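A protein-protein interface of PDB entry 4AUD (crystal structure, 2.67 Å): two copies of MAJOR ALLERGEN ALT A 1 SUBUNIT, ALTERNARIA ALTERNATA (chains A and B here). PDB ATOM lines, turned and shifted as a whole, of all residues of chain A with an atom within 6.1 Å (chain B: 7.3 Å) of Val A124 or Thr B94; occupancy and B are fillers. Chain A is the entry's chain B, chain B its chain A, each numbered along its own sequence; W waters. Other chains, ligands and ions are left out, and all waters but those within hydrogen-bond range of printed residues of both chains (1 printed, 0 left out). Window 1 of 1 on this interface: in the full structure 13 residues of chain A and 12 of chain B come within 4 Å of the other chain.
Of the 20 printed residues of chain B, 3 touch a printed residue of chain A. Printed residues of chain B that touch a printed residue of chain A: His B57, Leu B80 and Thr B94. Hydrophobic or aromatic side chains of chain B that line the printed part of chain A: His B57 and Leu B80. Among the printed residues, 4 pairs touch across the chains. Among the printed residues, no Asp or Glu carboxylate lies within 4 Å of a Lys or Arg side-chain nitrogen of the other chain.
Thr A94 touches its own counterpart, Thr B94. 5 positions are printed for both chains.
O of Leu B80 lies within hydrogen-bond range of N of Ser B71 (2.9 Å). The backbone NH (N) of Val A92 is in hydrogen-bond range of the backbone carbonyl oxygen (O) of Val A124 (2.9 Å).
Val A124 touches just one residue of chain B: Thr B94 (3.5 Å). Of the printed residues of chain A, His B57 touches Thr A125. Of the printed residues of chain B, Thr A125 touches His B57 and Leu B80. Of the printed residues of chain B, Thr A94 touches Thr B94. Printed residues of chain A within 4 Å of Leu B80: Thr A125 (3.8 Å). Ile B15 touches none of the printed residues of chain A. The nearest residue of chain A that does not touch Thr B94 is Thr A122 (4.7 Å).
Among the printed residues, pairs that only touch across the chains: Thr A94 with Thr B94 (3.7 Å), Val A124 with Thr B94 (3.5 Å), Thr A125 with His B57 (3.5 Å) and Thr A125 with Leu B80 (3.8 Å).
Water W1 bridges O of Thr A125 (2.6 Å) and OG of Ser B71 (2.6 Å).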
ATOM      1  N   THR A  90       1.865  -4.069 -36.423  1.00  0.00           N
ATOM      2  CA  THR A  90       1.192  -4.071 -35.126  1.00  0.00           C
ATOM      3  C   THR A  90       1.853  -3.093 -34.145  1.00  0.00           C
ATOM      4  O   THR A  90       3.073  -3.074 -33.976  1.00  0.00           O
ATOM      5  CB  THR A  90       1.101  -5.488 -34.525  1.00  0.00           C
ATOM      6  OG1 THR A  90       0.232  -6.287 -35.332  1.00  0.00           O
ATOM      7  CG2 THR A  90       0.557  -5.449 -33.098  1.00  0.00           C
ATOM      8  N   TYR A  91       1.028  -2.269 -33.514  1.00  0.00           N
ATOM      9  CA  TYR A  91       1.493  -1.354 -32.485  1.00  0.00           C
ATOM     10  C   TYR A  91       1.232  -1.892 -31.083  1.00  0.00           C
ATOM     11  O   TYR A  91       0.269  -2.617 -30.854  1.00  0.00           O
ATOM     12  CB  TYR A  91       0.805  -0.008 -32.653  1.00  0.00           C
ATOM     13  CG  TYR A  91       1.125   0.601 -33.986  1.00  0.00           C
ATOM     14  CD1 TYR A  91       2.435   0.606 -34.464  1.00  0.00           C
ATOM     15  CD2 TYR A  91       0.119   1.142 -34.789  1.00  0.00           C
ATOM     16  CE1 TYR A  91       2.736   1.150 -35.685  1.00  0.00           C
ATOM     17  CE2 TYR A  91       0.411   1.682 -36.014  1.00  0.00           C
ATOM     18  CZ  TYR A  91       1.720   1.685 -36.460  1.00  0.00           C
ATOM     19  OH  TYR A  91       2.010   2.235 -37.684  1.00  0.00           O
ATOM     20  N   VAL A  92       2.103  -1.538 -30.146  1.00  0.00           N
ATOM     21  CA  VAL A  92       1.869  -1.848 -28.744  1.00  0.00           C
ATOM     22  C   VAL A  92       2.243  -0.648 -27.894  1.00  0.00           C
ATOM     23  O   VAL A  92       3.044   0.184 -28.310  1.00  0.00           O
ATOM     24  CB  VAL A  92       2.685  -3.058 -28.307  1.00  0.00           C
ATOM     25  CG1 VAL A  92       2.138  -4.320 -28.966  1.00  0.00           C
ATOM     26  CG2 VAL A  92       4.141  -2.846 -28.685  1.00  0.00           C
ATOM     27  N   ALA A  93       1.652  -0.552 -26.711  1.00  0.00           N
ATOM     28  CA  ALA A  93       1.979   0.531 -25.795  1.00  0.00           C
ATOM     29  C   ALA A  93       1.728   0.098 -24.370  1.00  0.00           C
ATOM     30  O   ALA A  93       0.825  -0.684 -24.124  1.00  0.00           O
ATOM     31  CB  ALA A  93       1.146   1.759 -26.115  1.00  0.00           C
ATOM     32  N   THR A  94       2.525   0.612 -23.439  1.00  0.00           N
ATOM     33  CA  THR A  94       2.277   0.408 -22.013  1.00  0.00           C
ATOM     34  C   THR A  94       1.816   1.698 -21.338  1.00  0.00           C
ATOM     35  O   THR A  94       2.249   2.793 -21.698  1.00  0.00           O
ATOM     36  CB  THR A  94       3.540  -0.079 -21.272  1.00  0.00           C
ATOM     37  OG1 THR A  94       4.375   1.043 -20.942  1.00  0.00           O
ATOM     38  CG2 THR A  94       4.313  -1.052 -22.130  1.00  0.00           C
ATOM     39  N   THR A 122       2.783   6.217 -26.037  1.00  0.00           N
ATOM     40  CA  THR A 122       3.444   6.233 -27.322  1.00  0.00           C
ATOM     41  C   THR A 122       3.450   4.827 -27.904  1.00  0.00           C
ATOM     42  O   THR A 122       3.783   3.849 -27.225  1.00  0.00           O
ATOM     43  CB  THR A 122       4.874   6.755 -27.197  1.00  0.00           C
ATOM     44  OG1 THR A 122       4.841   8.180 -27.050  1.00  0.00           O
ATOM     45  CG2 THR A 122       5.682   6.400 -28.427  1.00  0.00           C
ATOM     46  N   LEU A 123       3.071   4.745 -29.171  1.00  0.00           N
ATOM     47  CA  LEU A 123       3.006   3.489 -29.890  1.00  0.00           C
ATOM     48  C   LEU A 123       4.373   3.106 -30.423  1.00  0.00           C
ATOM     49  O   LEU A 123       5.098   3.947 -30.965  1.00  0.00           O
ATOM     50  CB  LEU A 123       2.022   3.616 -31.044  1.00  0.00           C
ATOM     51  CG  LEU A 123       0.542   3.372 -30.717  1.00  0.00           C
ATOM     52  CD1 LEU A 123       0.180   3.688 -29.275  1.00  0.00           C
ATOM     53  CD2 LEU A 123      -0.312   4.191 -31.659  1.00  0.00           C
ATOM     54  N   VAL A 124       4.736   1.841 -30.240  1.00  0.00           N
ATOM     55  CA  VAL A 124       5.913   1.288 -30.900  1.00  0.00           C
ATOM     56  C   VAL A 124       5.489   0.103 -31.758  1.00  0.00           C
ATOM     57  O   VAL A 124       4.465  -0.550 -31.500  1.00  0.00           O
ATOM     58  CB  VAL A 124       7.035   0.859 -29.914  1.00  0.00           C
ATOM     59  CG1 VAL A 124       7.831   2.055 -29.451  1.00  0.00           C
ATOM     60  CG2 VAL A 124       6.465   0.130 -28.736  1.00  0.00           C
ATOM     61  N   THR A 125       6.274  -0.164 -32.789  1.00  0.00           N
ATOM     62  CA  THR A 125       5.967  -1.261 -33.678  1.00  0.00           C
ATOM     63  C   THR A 125       6.492  -2.560 -33.096  1.00  0.00           C
ATOM     64  O   THR A 125       7.635  -2.648 -32.646  1.00  0.00           O
ATOM     65  CB  THR A 125       6.535  -1.022 -35.074  1.00  0.00           C
ATOM     66  OG1 THR A 125       6.096   0.266 -35.551  1.00  0.00           O
ATOM     67  CG2 THR A 125       6.068  -2.122 -36.017  1.00  0.00           C
ATOM     68  N   LEU A 126       5.621  -3.556 -33.089  1.00  0.00           N
ATOM     69  CA  LEU A 126       5.923  -4.883 -32.594  1.00  0.00           C
ATOM     70  C   LEU A 126       6.566  -5.700 -33.712  1.00  0.00           C
ATOM     71  O   LEU A 126       5.959  -5.875 -34.768  1.00  0.00           O
ATOM     72  CB  LEU A 126       4.606  -5.542 -32.214  1.00  0.00           C
ATOM     73  CG  LEU A 126       4.541  -6.555 -31.070  1.00  0.00           C
ATOM     74  CD1 LEU A 126       3.475  -7.599 -31.406  1.00  0.00           C
ATOM     75  CD2 LEU A 126       5.885  -7.196 -30.769  1.00  0.00           C
ATOM     76  N   ILE B  15      17.017   3.807 -18.202  1.00  0.00           N
ATOM     77  CA  ILE B  15      17.749   3.556 -19.421  1.00  0.00           C
ATOM     78  C   ILE B  15      18.596   4.771 -19.671  1.00  0.00           C
ATOM     79  O   ILE B  15      18.088   5.911 -19.648  1.00  0.00           O
ATOM     80  CB  ILE B  15      16.842   3.395 -20.632  1.00  0.00           C
ATOM     81  CG1 ILE B  15      15.689   2.437 -20.338  1.00  0.00           C
ATOM     82  CG2 ILE B  15      17.665   2.900 -21.802  1.00  0.00           C
ATOM     83  CD1 ILE B  15      16.148   1.040 -19.995  1.00  0.00           C
ATOM     84  N   HIS B  57      12.670  -2.395 -35.925  1.00  0.00           N
ATOM     85  CA  HIS B  57      11.546  -3.277 -35.611  1.00  0.00           C
ATOM     86  C   HIS B  57      11.871  -4.760 -35.757  1.00  0.00           C
ATOM     87  O   HIS B  57      11.121  -5.518 -36.363  1.00  0.00           O
ATOM     88  CB  HIS B  57      10.353  -2.920 -36.486  1.00  0.00           C
ATOM     89  CG  HIS B  57      10.035  -1.466 -36.474  1.00  0.00           C
ATOM     90  ND1 HIS B  57       9.740  -0.751 -37.617  1.00  0.00           N
ATOM     91  CD2 HIS B  57       9.997  -0.581 -35.455  1.00  0.00           C
ATOM     92  CE1 HIS B  57       9.519   0.509 -37.298  1.00  0.00           C
ATOM     93  NE2 HIS B  57       9.668   0.641 -35.991  1.00  0.00           N
ATOM     94  N   SER B  71      13.972  -4.228 -29.444  1.00  0.00           N
ATOM     95  CA  SER B  71      13.715  -3.821 -30.802  1.00  0.00           C
ATOM     96  C   SER B  71      13.808  -2.312 -30.815  1.00  0.00           C
ATOM     97  O   SER B  71      13.487  -1.659 -29.830  1.00  0.00           O
ATOM     98  CB  SER B  71      12.340  -4.279 -31.238  1.00  0.00           C
ATOM     99  OG  SER B  71      12.040  -3.729 -32.507  1.00  0.00           O
ATOM    100  N   GLY B  73      13.324   1.385 -33.170  1.00  0.00           N
ATOM    101  CA  GLY B  73      12.827   2.057 -34.349  1.00  0.00           C
ATOM    102  C   GLY B  73      13.555   3.374 -34.444  1.00  0.00           C
ATOM    103  O   GLY B  73      13.242   4.309 -33.714  1.00  0.00           O
ATOM    104  N   ARG B  76      11.422   6.946 -34.772  1.00  0.00           N
ATOM    105  CA  ARG B  76      11.044   7.853 -33.701  1.00  0.00           C
ATOM    106  C   ARG B  76      11.858   7.535 -32.442  1.00  0.00           C
ATOM    107  O   ARG B  76      11.492   7.912 -31.318  1.00  0.00           O
ATOM    108  CB  ARG B  76       9.535   7.770 -33.426  1.00  0.00           C
ATOM    109  CG  ARG B  76       8.678   8.688 -34.289  1.00  0.00           C
ATOM    110  CD  ARG B  76       7.386   9.119 -33.570  1.00  0.00           C
ATOM    111  NE  ARG B  76       6.742  10.289 -34.192  1.00  0.00           N
ATOM    112  CZ  ARG B  76       5.681  10.937 -33.694  1.00  0.00           C
ATOM    113  NH1 ARG B  76       5.121  10.545 -32.556  1.00  0.00           N
ATOM    114  NH2 ARG B  76       5.173  11.986 -34.336  1.00  0.00           N
ATOM    115  N   SER B  77      12.971   6.837 -32.636  1.00  0.00           N
ATOM    116  CA  SER B  77      13.836   6.463 -31.517  1.00  0.00           C
ATOM    117  C   SER B  77      13.065   5.699 -30.451  1.00  0.00           C
ATOM    118  O   SER B  77      13.231   5.921 -29.255  1.00  0.00           O
ATOM    119  CB  SER B  77      14.514   7.690 -30.927  1.00  0.00           C
ATOM    120  OG  SER B  77      15.303   8.309 -31.923  1.00  0.00           O
ATOM    121  N   GLY B  78      12.213   4.792 -30.910  1.00  0.00           N
ATOM    122  CA  GLY B  78      11.406   3.998 -30.020  1.00  0.00           C
ATOM    123  C   GLY B  78      12.128   2.728 -29.647  1.00  0.00           C
ATOM    124  O   GLY B  78      12.733   2.056 -30.492  1.00  0.00           O
ATOM    125  N   LEU B  79      12.069   2.399 -28.365  1.00  0.00           N
ATOM    126  CA  LEU B  79      12.680   1.188 -27.863  1.00  0.00           C
ATOM    127  C   LEU B  79      11.635   0.257 -27.240  1.00  0.00           C
ATOM    128  O   LEU B  79      10.752   0.690 -26.484  1.00  0.00           O
ATOM    129  CB  LEU B  79      13.739   1.541 -26.839  1.00  0.00           C
ATOM    130  CG  LEU B  79      14.311   0.298 -26.172  1.00  0.00           C
ATOM    131  CD1 LEU B  79      15.215  -0.407 -27.152  1.00  0.00           C
ATOM    132  CD2 LEU B  79      15.044   0.659 -24.898  1.00  0.00           C
ATOM    133  N   LEU B  80      11.735  -1.026 -27.577  1.00  0.00           N
ATOM    134  CA  LEU B  80      10.860  -2.048 -27.033  1.00  0.00           C
ATOM    135  C   LEU B  80      11.753  -3.053 -26.345  1.00  0.00           C
ATOM    136  O   LEU B  80      12.640  -3.615 -26.960  1.00  0.00           O
ATOM    137  CB  LEU B  80      10.125  -2.735 -28.163  1.00  0.00           C
ATOM    138  CG  LEU B  80       8.681  -3.170 -27.984  1.00  0.00           C
ATOM    139  CD1 LEU B  80       8.326  -3.996 -29.185  1.00  0.00           C
ATOM    140  CD2 LEU B  80       8.525  -3.981 -26.751  1.00  0.00           C
ATOM    141  N   LEU B  81      11.514  -3.288 -25.068  1.00  0.00           N
ATOM    142  CA  LEU B  81      12.400  -4.124 -24.279  1.00  0.00           C
ATOM    143  C   LEU B  81      11.662  -5.356 -23.768  1.00  0.00           C
ATOM    144  O   LEU B  81      10.549  -5.241 -23.265  1.00  0.00           O
ATOM    145  CB  LEU B  81      12.920  -3.307 -23.099  1.00  0.00           C
ATOM    146  CG  LEU B  81      14.376  -3.462 -22.697  1.00  0.00           C
ATOM    147  CD1 LEU B  81      14.470  -3.354 -21.197  1.00  0.00           C
ATOM    148  CD2 LEU B  81      14.932  -4.789 -23.175  1.00  0.00           C
ATOM    149  N   VAL B  92       7.561  -6.718 -20.358  1.00  0.00           N
ATOM    150  CA  VAL B  92       7.926  -5.812 -21.454  1.00  0.00           C
ATOM    151  C   VAL B  92       7.843  -4.349 -21.036  1.00  0.00           C
ATOM    152  O   VAL B  92       7.208  -4.016 -20.025  1.00  0.00           O
ATOM    153  CB  VAL B  92       7.034  -6.019 -22.681  1.00  0.00           C
ATOM    154  CG1 VAL B  92       7.278  -7.417 -23.279  1.00  0.00           C
ATOM    155  CG2 VAL B  92       5.569  -5.835 -22.284  1.00  0.00           C
ATOM    156  N   ALA B  93       8.484  -3.483 -21.819  1.00  0.00           N
ATOM    157  CA  ALA B  93       8.495  -2.046 -21.547  1.00  0.00           C
ATOM    158  C   ALA B  93       8.793  -1.267 -22.820  1.00  0.00           C
ATOM    159  O   ALA B  93       9.288  -1.843 -23.797  1.00  0.00           O
ATOM    160  CB  ALA B  93       9.532  -1.714 -20.487  1.00  0.00           C
ATOM    161  N   THR B  94       8.495   0.035 -22.792  1.00  0.00           N
ATOM    162  CA  THR B  94       8.663   0.927 -23.947  1.00  0.00           C
ATOM    163  C   THR B  94       9.260   2.270 -23.543  1.00  0.00           C
ATOM    164  O   THR B  94       8.918   2.851 -22.511  1.00  0.00           O
ATOM    165  CB  THR B  94       7.323   1.222 -24.713  1.00  0.00           C
ATOM    166  OG1 THR B  94       6.420   1.945 -23.866  1.00  0.00           O
ATOM    167  CG2 THR B  94       6.648  -0.054 -25.199  1.00  0.00           C
ATOM    168  N   ALA B  95      10.146   2.777 -24.385  1.00  0.00           N
ATOM    169  CA  ALA B  95      10.791   4.044 -24.114  1.00  0.00           C
ATOM    170  C   ALA B  95      11.093   4.771 -25.402  1.00  0.00           C
ATOM    171  O   ALA B  95      11.070   4.192 -26.490  1.00  0.00           O
ATOM    172  CB  ALA B  95      12.055   3.824 -23.356  1.00  0.00           C
ATOM    173  N   THR B  96      11.368   6.056 -25.264  1.00  0.00           N
ATOM    174  CA  THR B  96      11.881   6.841 -26.357  1.00  0.00           C
ATOM    175  C   THR B  96      13.261   7.325 -25.947  1.00  0.00           C
ATOM    176  O   THR B  96      13.432   7.858 -24.848  1.00  0.00           O
ATOM    177  CB  THR B  96      10.992   8.043 -26.599  1.00  0.00           C
ATOM    178  OG1 THR B  96       9.714   7.596 -27.090  1.00  0.00           O
ATOM    179  CG2 THR B  96      11.666   9.028 -27.596  1.00  0.00           C
ATOM    180  N   ALA B 119      15.865   7.776 -19.862  1.00  0.00           N
ATOM    181  CA  ALA B 119      14.471   7.342 -19.875  1.00  0.00           C
ATOM    182  C   ALA B 119      14.188   6.451 -18.668  1.00  0.00           C
ATOM    183  O   ALA B 119      15.073   5.777 -18.148  1.00  0.00           O
ATOM    184  CB  ALA B 119      14.142   6.607 -21.171  1.00  0.00           C
ATOM    185  N   TYR B 120      12.945   6.456 -18.219  1.00  0.00           N
ATOM    186  CA  TYR B 120      12.550   5.633 -17.087  1.00  0.00           C
ATOM    187  C   TYR B 120      11.407   4.722 -17.513  1.00  0.00           C
ATOM    188  O   TYR B 120      10.342   5.196 -17.874  1.00  0.00           O
ATOM    189  CB  TYR B 120      12.206   6.511 -15.876  1.00  0.00           C
ATOM    190  CG  TYR B 120      13.428   7.262 -15.344  1.00  0.00           C
ATOM    191  CD1 TYR B 120      13.869   8.437 -15.956  1.00  0.00           C
ATOM    192  CD2 TYR B 120      14.162   6.780 -14.252  1.00  0.00           C
ATOM    193  CE1 TYR B 120      14.991   9.117 -15.495  1.00  0.00           C
ATOM    194  CE2 TYR B 120      15.297   7.463 -13.780  1.00  0.00           C
ATOM    195  CZ  TYR B 120      15.700   8.631 -14.408  1.00  0.00           C
ATOM    196  OH  TYR B 120      16.811   9.321 -13.970  1.00  0.00           O
ATOM    197  N   ILE B 121      11.650   3.413 -17.523  1.00  0.00           N
ATOM    198  CA  ILE B 121      10.633   2.490 -18.010  1.00  0.00           C
ATOM    199  C   ILE B 121       9.913   1.756 -16.906  1.00  0.00           C
ATOM    200  O   ILE B 121      10.431   1.546 -15.815  1.00  0.00           O
ATOM    201  CB  ILE B 121      11.214   1.438 -18.933  1.00  0.00           C
ATOM    202  CG1 ILE B 121      12.182   0.561 -18.153  1.00  0.00           C
ATOM    203  CG2 ILE B 121      11.901   2.093 -20.114  1.00  0.00           C
ATOM    204  CD1 ILE B 121      12.747  -0.561 -18.960  1.00  0.00           C
ATOM    205  N   THR B 122       8.687   1.370 -17.206  1.00  0.00           N
ATOM    206  CA  THR B 122       7.907   0.570 -16.289  1.00  0.00           C
ATOM    207  C   THR B 122       7.596  -0.754 -16.946  1.00  0.00           C
ATOM    208  O   THR B 122       7.052  -0.788 -18.049  1.00  0.00           O
ATOM    209  CB  THR B 122       6.619   1.267 -15.907  1.00  0.00           C
ATOM    210  OG1 THR B 122       6.934   2.480 -15.214  1.00  0.00           O
ATOM    211  CG2 THR B 122       5.810   0.386 -14.994  1.00  0.00           C
ATOM    212  N   LEU B 123       7.975  -1.835 -16.269  1.00  0.00           N
ATOM    213  CA  LEU B 123       7.789  -3.177 -16.792  1.00  0.00           C
ATOM    214  C   LEU B 123       6.384  -3.656 -16.517  1.00  0.00           C
ATOM    215  O   LEU B 123       5.864  -3.472 -15.422  1.00  0.00           O
ATOM    216  CB  LEU B 123       8.775  -4.141 -16.156  1.00  0.00           C
ATOM    217  CG  LEU B 123      10.138  -4.217 -16.834  1.00  0.00           C
ATOM    218  CD1 LEU B 123      10.865  -2.898 -16.729  1.00  0.00           C
ATOM    219  CD2 LEU B 123      10.953  -5.296 -16.184  1.00  0.00           C
HETATM  220  O   HOH W   1      10.115  -1.991 -32.456  1.00  0.00           O
